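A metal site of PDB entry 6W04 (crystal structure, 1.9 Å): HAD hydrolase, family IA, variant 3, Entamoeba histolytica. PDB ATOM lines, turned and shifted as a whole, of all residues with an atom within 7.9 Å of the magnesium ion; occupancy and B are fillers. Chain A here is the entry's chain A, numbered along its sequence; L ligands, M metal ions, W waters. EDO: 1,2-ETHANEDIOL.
Merely in contact with the magnesium ion: Glu 168 (3.97 Å). The nearest printed residue that does not touch the magnesium ion is Thr 11 (4.1 Å).
The magnesium ion is bound by an oxygen (O1) of the ligand, the side-chain carboxylate (OD2) of Asp 7, the side-chain carboxylate (OD2) of Asp 169, the backbone carbonyl oxygen (O) of Asn 9, water W2 and water W1.
Water W2 lies within hydrogen-bond range of OE1 of Glu 168 (2.6 Å), OG1 of Thr 170 (3.2 Å) and NZ of Lys 144 (3.4 Å).
N of Asp 7 sits at hydrogen-bond distance from O of Phe 167 (3.1 Å). The side-chain hydroxyl (OG1) of Thr 109 is in hydrogen-bond range of the side-chain amide oxygen (OD1) of Asn 9, at 3.1 Å. The side-chain amino group of Lys 144 is in salt-bridge range of the side-chain carboxylate of Glu 168 (2.6 Å). The side-chain hydroxyl (OG1) of Thr 11 sits close to the side-chain carboxylate (OD2) of Asp 7, 3.0 Å away. The side-chain hydroxyl of Thr 11 sits at hydrogen-bond distance from the backbone NH of Asp 169. OE2 of Glu 168 is in hydrogen-bond range of OH of Tyr 150, 2.5 Å away. The side-chain amide nitrogen of Asn 9 sits at hydrogen-bond distance from the side-chain carboxylate of Asp 15 (2.7 Å). The side-chain carboxylate (OD1) of Asp 7 is in salt-bridge range of the side-chain amino group (NZ) of Lys 144 (2.8 Å).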
ATOM      1  N   ASP A   7      -2.213  -1.333  14.307  1.00  0.00           N
ATOM      2  CA  ASP A   7      -1.714  -1.270  15.680  1.00  0.00           C
ATOM      3  C   ASP A   7      -1.102  -2.607  16.037  1.00  0.00           C
ATOM      4  O   ASP A   7      -1.427  -3.632  15.430  1.00  0.00           O
ATOM      5  CB  ASP A   7      -2.860  -0.951  16.629  1.00  0.00           C
ATOM      6  CG  ASP A   7      -2.422  -0.888  18.075  1.00  0.00           C
ATOM      7  OD1 ASP A   7      -1.405  -0.214  18.364  1.00  0.00           O
ATOM      8  OD2 ASP A   7      -3.126  -1.477  18.923  1.00  0.00           O
ATOM      9  N   PHE A   8      -0.220  -2.638  17.040  1.00  0.00           N
ATOM     10  CA  PHE A   8       0.433  -3.901  17.355  1.00  0.00           C
ATOM     11  C   PHE A   8      -0.110  -4.528  18.648  1.00  0.00           C
ATOM     12  O   PHE A   8      -0.796  -5.553  18.579  1.00  0.00           O
ATOM     13  CB  PHE A   8       1.942  -3.748  17.406  1.00  0.00           C
ATOM     14  CG  PHE A   8       2.658  -5.067  17.390  1.00  0.00           C
ATOM     15  CD1 PHE A   8       2.873  -5.748  16.203  1.00  0.00           C
ATOM     16  CD2 PHE A   8       3.019  -5.681  18.586  1.00  0.00           C
ATOM     17  CE1 PHE A   8       3.475  -6.988  16.190  1.00  0.00           C
ATOM     18  CE2 PHE A   8       3.646  -6.912  18.581  1.00  0.00           C
ATOM     19  CZ  PHE A   8       3.864  -7.571  17.383  1.00  0.00           C
ATOM     20  N   ASN A   9       0.143  -3.921  19.814  1.00  0.00           N
ATOM     21  CA  ASN A   9      -0.293  -4.502  21.085  1.00  0.00           C
ATOM     22  C   ASN A   9      -1.807  -4.541  21.177  1.00  0.00           C
ATOM     23  O   ASN A   9      -2.478  -3.523  21.030  1.00  0.00           O
ATOM     24  CB  ASN A   9       0.276  -3.681  22.243  1.00  0.00           C
ATOM     25  CG  ASN A   9       1.781  -3.577  22.185  1.00  0.00           C
ATOM     26  OD1 ASN A   9       2.341  -2.554  21.760  1.00  0.00           O
ATOM     27  ND2 ASN A   9       2.442  -4.658  22.545  1.00  0.00           N
ATOM     28  N   GLY A  10      -2.347  -5.725  21.462  1.00  0.00           N
ATOM     29  CA  GLY A  10      -3.787  -5.910  21.581  1.00  0.00           C
ATOM     30  C   GLY A  10      -4.495  -6.067  20.261  1.00  0.00           C
ATOM     31  O   GLY A  10      -5.670  -6.424  20.240  1.00  0.00           O
ATOM     32  N   THR A  11      -3.800  -5.849  19.148  1.00  0.00           N
ATOM     33  CA  THR A  11      -4.364  -5.930  17.809  1.00  0.00           C
ATOM     34  C   THR A  11      -3.706  -7.045  17.008  1.00  0.00           C
ATOM     35  O   THR A  11      -4.403  -7.973  16.569  1.00  0.00           O
ATOM     36  CB  THR A  11      -4.191  -4.556  17.118  1.00  0.00           C
ATOM     37  OG1 THR A  11      -4.992  -3.564  17.786  1.00  0.00           O
ATOM     38  CG2 THR A  11      -4.589  -4.618  15.641  1.00  0.00           C
ATOM     39  N   LEU A  12      -2.386  -6.997  16.799  1.00  0.00           N
ATOM     40  CA  LEU A  12      -1.686  -8.084  16.112  1.00  0.00           C
ATOM     41  C   LEU A  12      -1.260  -9.198  17.047  1.00  0.00           C
ATOM     42  O   LEU A  12      -1.110 -10.347  16.608  1.00  0.00           O
ATOM     43  CB  LEU A  12      -0.466  -7.542  15.365  1.00  0.00           C
ATOM     44  CG  LEU A  12      -0.793  -6.862  14.029  1.00  0.00           C
ATOM     45  CD1 LEU A  12       0.438  -6.215  13.413  1.00  0.00           C
ATOM     46  CD2 LEU A  12      -1.430  -7.881  13.024  1.00  0.00           C
ATOM     47  N   ILE A  13      -1.048  -8.909  18.332  1.00  0.00           N
ATOM     48  CA  ILE A  13      -0.868  -9.945  19.346  1.00  0.00           C
ATOM     49  C   ILE A  13      -1.808  -9.643  20.517  1.00  0.00           C
ATOM     50  O   ILE A  13      -2.021  -8.484  20.865  1.00  0.00           O
ATOM     51  CB  ILE A  13       0.597 -10.048  19.828  1.00  0.00           C
ATOM     52  CG1 ILE A  13       1.101  -8.742  20.471  1.00  0.00           C
ATOM     53  CG2 ILE A  13       1.522 -10.470  18.670  1.00  0.00           C
ATOM     54  CD1 ILE A  13       2.518  -8.920  21.155  1.00  0.00           C
ATOM     55  N   ASP A  15      -1.775  -9.475  23.818  1.00  0.00           N
ATOM     56  CA  ASP A  15      -0.840  -9.452  24.946  1.00  0.00           C
ATOM     57  C   ASP A  15      -1.372  -8.675  26.143  1.00  0.00           C
ATOM     58  O   ASP A  15      -0.630  -8.466  27.101  1.00  0.00           O
ATOM     59  CB  ASP A  15       0.511  -8.883  24.514  1.00  0.00           C
ATOM     60  CG  ASP A  15       0.426  -7.441  23.988  1.00  0.00           C
ATOM     61  OD1 ASP A  15      -0.680  -6.995  23.595  1.00  0.00           O
ATOM     62  OD2 ASP A  15       1.470  -6.760  23.961  1.00  0.00           O
ATOM     63  N   THR A  16      -2.638  -8.264  26.124  1.00  0.00           N
ATOM     64  CA  THR A  16      -3.135  -7.551  27.307  1.00  0.00           C
ATOM     65  C   THR A  16      -3.015  -8.376  28.594  1.00  0.00           C
ATOM     66  O   THR A  16      -2.556  -7.806  29.604  1.00  0.00           O
ATOM     67  CB  THR A  16      -4.570  -7.086  27.059  1.00  0.00           C
ATOM     68  OG1 THR A  16      -4.569  -6.180  25.953  1.00  0.00           O
ATOM     69  CG2 THR A  16      -5.113  -6.362  28.331  1.00  0.00           C
ATOM     70  N   ALA A 108       1.976   0.618  13.397  1.00  0.00           N
ATOM     71  CA  ALA A 108       2.174   1.750  14.281  1.00  0.00           C
ATOM     72  C   ALA A 108       1.936   1.260  15.700  1.00  0.00           C
ATOM     73  O   ALA A 108       0.970   0.521  15.948  1.00  0.00           O
ATOM     74  CB  ALA A 108       1.240   2.904  13.944  1.00  0.00           C
ATOM     75  N   THR A 109       2.814   1.609  16.633  1.00  0.00           N
ATOM     76  CA  THR A 109       2.626   1.156  17.994  1.00  0.00           C
ATOM     77  C   THR A 109       3.030   2.266  18.944  1.00  0.00           C
ATOM     78  O   THR A 109       3.904   3.078  18.628  1.00  0.00           O
ATOM     79  CB  THR A 109       3.424  -0.133  18.267  1.00  0.00           C
ATOM     80  OG1 THR A 109       3.351  -0.487  19.651  1.00  0.00           O
ATOM     81  CG2 THR A 109       4.877   0.024  17.875  1.00  0.00           C
ATOM     82  N   SER A 110       2.380   2.304  20.102  1.00  0.00           N
ATOM     83  CA  SER A 110       2.802   3.179  21.193  1.00  0.00           C
ATOM     84  C   SER A 110       4.043   2.657  21.902  1.00  0.00           C
ATOM     85  O   SER A 110       4.595   3.371  22.742  1.00  0.00           O
ATOM     86  CB  SER A 110       1.701   3.331  22.238  1.00  0.00           C
ATOM     87  OG  SER A 110       0.505   3.848  21.699  1.00  0.00           O
ATOM     88  N   LYS A 144      -1.311   8.489  21.236  1.00  0.00           N
ATOM     89  CA  LYS A 144      -2.751   8.309  21.163  1.00  0.00           C
ATOM     90  C   LYS A 144      -3.403   8.859  22.432  1.00  0.00           C
ATOM     91  O   LYS A 144      -2.869   8.673  23.531  1.00  0.00           O
ATOM     92  CB  LYS A 144      -3.097   6.835  21.003  1.00  0.00           C
ATOM     93  CG  LYS A 144      -2.358   6.136  19.880  1.00  0.00           C
ATOM     94  CD  LYS A 144      -2.514   4.636  20.004  1.00  0.00           C
ATOM     95  CE  LYS A 144      -1.791   3.938  18.906  1.00  0.00           C
ATOM     96  NZ  LYS A 144      -2.028   2.481  18.935  1.00  0.00           N
ATOM     97  N   TYR A 150      -0.731   8.129  13.391  1.00  0.00           N
ATOM     98  CA  TYR A 150      -1.256   7.573  12.139  1.00  0.00           C
ATOM     99  C   TYR A 150      -0.975   8.467  10.940  1.00  0.00           C
ATOM    100  O   TYR A 150      -0.777   7.951   9.827  1.00  0.00           O
ATOM    101  CB  TYR A 150      -2.756   7.253  12.276  1.00  0.00           C
ATOM    102  CG  TYR A 150      -2.946   5.998  13.096  1.00  0.00           C
ATOM    103  CD1 TYR A 150      -2.323   4.813  12.705  1.00  0.00           C
ATOM    104  CD2 TYR A 150      -3.684   6.000  14.276  1.00  0.00           C
ATOM    105  CE1 TYR A 150      -2.447   3.650  13.454  1.00  0.00           C
ATOM    106  CE2 TYR A 150      -3.814   4.829  15.054  1.00  0.00           C
ATOM    107  CZ  TYR A 150      -3.182   3.666  14.635  1.00  0.00           C
ATOM    108  OH  TYR A 150      -3.287   2.486  15.366  1.00  0.00           O
ATOM    109  N   PHE A 167      -6.539  -0.774  11.987  1.00  0.00           N
ATOM    110  CA  PHE A 167      -6.998  -1.805  12.923  1.00  0.00           C
ATOM    111  C   PHE A 167      -6.519  -1.415  14.317  1.00  0.00           C
ATOM    112  O   PHE A 167      -5.321  -1.189  14.524  1.00  0.00           O
ATOM    113  CB  PHE A 167      -6.451  -3.185  12.550  1.00  0.00           C
ATOM    114  CG  PHE A 167      -7.072  -3.781  11.300  1.00  0.00           C
ATOM    115  CD1 PHE A 167      -6.381  -3.809  10.100  1.00  0.00           C
ATOM    116  CD2 PHE A 167      -8.331  -4.357  11.349  1.00  0.00           C
ATOM    117  CE1 PHE A 167      -6.945  -4.386   8.951  1.00  0.00           C
ATOM    118  CE2 PHE A 167      -8.916  -4.931  10.218  1.00  0.00           C
ATOM    119  CZ  PHE A 167      -8.209  -4.933   9.011  1.00  0.00           C
ATOM    120  N   GLU A 168      -7.446  -1.347  15.273  1.00  0.00           N
ATOM    121  CA  GLU A 168      -7.110  -0.846  16.596  1.00  0.00           C
ATOM    122  C   GLU A 168      -7.957  -1.591  17.613  1.00  0.00           C
ATOM    123  O   GLU A 168      -9.027  -2.101  17.284  1.00  0.00           O
ATOM    124  CB  GLU A 168      -7.362   0.661  16.689  1.00  0.00           C
ATOM    125  CG  GLU A 168      -6.150   1.509  16.478  1.00  0.00           C
ATOM    126  CD  GLU A 168      -5.246   1.497  17.698  1.00  0.00           C
ATOM    127  OE1 GLU A 168      -5.551   0.765  18.681  1.00  0.00           O
ATOM    128  OE2 GLU A 168      -4.237   2.235  17.673  1.00  0.00           O
ATOM    129  N   ASP A 169      -7.476  -1.648  18.872  1.00  0.00           N
ATOM    130  CA  ASP A 169      -8.159  -2.405  19.924  1.00  0.00           C
ATOM    131  C   ASP A 169      -8.573  -1.572  21.132  1.00  0.00           C
ATOM    132  O   ASP A 169      -9.202  -2.122  22.045  1.00  0.00           O
ATOM    133  CB  ASP A 169      -7.279  -3.558  20.420  1.00  0.00           C
ATOM    134  CG  ASP A 169      -6.046  -3.078  21.181  1.00  0.00           C
ATOM    135  OD1 ASP A 169      -5.883  -3.450  22.363  1.00  0.00           O
ATOM    136  OD2 ASP A 169      -5.239  -2.344  20.580  1.00  0.00           O
ATOM    137  N   THR A 170      -8.245  -0.281  21.176  1.00  0.00           N
ATOM    138  CA  THR A 170      -8.565   0.544  22.334  1.00  0.00           C
ATOM    139  C   THR A 170      -9.339   1.786  21.929  1.00  0.00           C
ATOM    140  O   THR A 170      -9.320   2.216  20.771  1.00  0.00           O
ATOM    141  CB  THR A 170      -7.308   0.999  23.071  1.00  0.00           C
ATOM    142  OG1 THR A 170      -6.537   1.830  22.184  1.00  0.00           O
ATOM    143  CG2 THR A 170      -6.472  -0.214  23.524  1.00  0.00           C
ATOM    144  N   GLY A 173      -6.900   4.499  20.772  1.00  0.00           N
ATOM    145  CA  GLY A 173      -6.374   4.208  19.438  1.00  0.00           C
ATOM    146  C   GLY A 173      -7.405   4.381  18.350  1.00  0.00           C
ATOM    147  O   GLY A 173      -7.089   4.838  17.236  1.00  0.00           O
ATOM    148  N   SER A 189     -10.154  -7.775  21.019  1.00  0.00           N
ATOM    149  CA  SER A 189      -9.292  -8.559  21.903  1.00  0.00           C
ATOM    150  C   SER A 189      -9.620  -8.351  23.373  1.00  0.00           C
ATOM    151  O   SER A 189      -9.448  -9.271  24.175  1.00  0.00           O
ATOM    152  CB  SER A 189      -7.817  -8.236  21.657  1.00  0.00           C
ATOM    153  OG  SER A 189      -7.568  -6.861  21.871  1.00  0.00           O
HETATM  154  C1  EDO L   1      -1.191  -0.414  22.835  1.00  0.00           C
HETATM  155  O1  EDO L   1      -1.541  -0.731  21.497  1.00  0.00           O
HETATM  156  C2  EDO L   1      -0.473   0.886  22.681  1.00  0.00           C
HETATM  157  O2  EDO L   1      -1.172   1.535  21.615  1.00  0.00           O
HETATM  158 MG    MG M   1      -3.325  -1.589  20.970  1.00  0.00          MG
HETATM  159  O   HOH W   1      -3.756  -2.021  23.079  1.00  0.00           O
HETATM  160  O   HOH W   2      -4.071   0.401  20.741  1.00  0.00           O
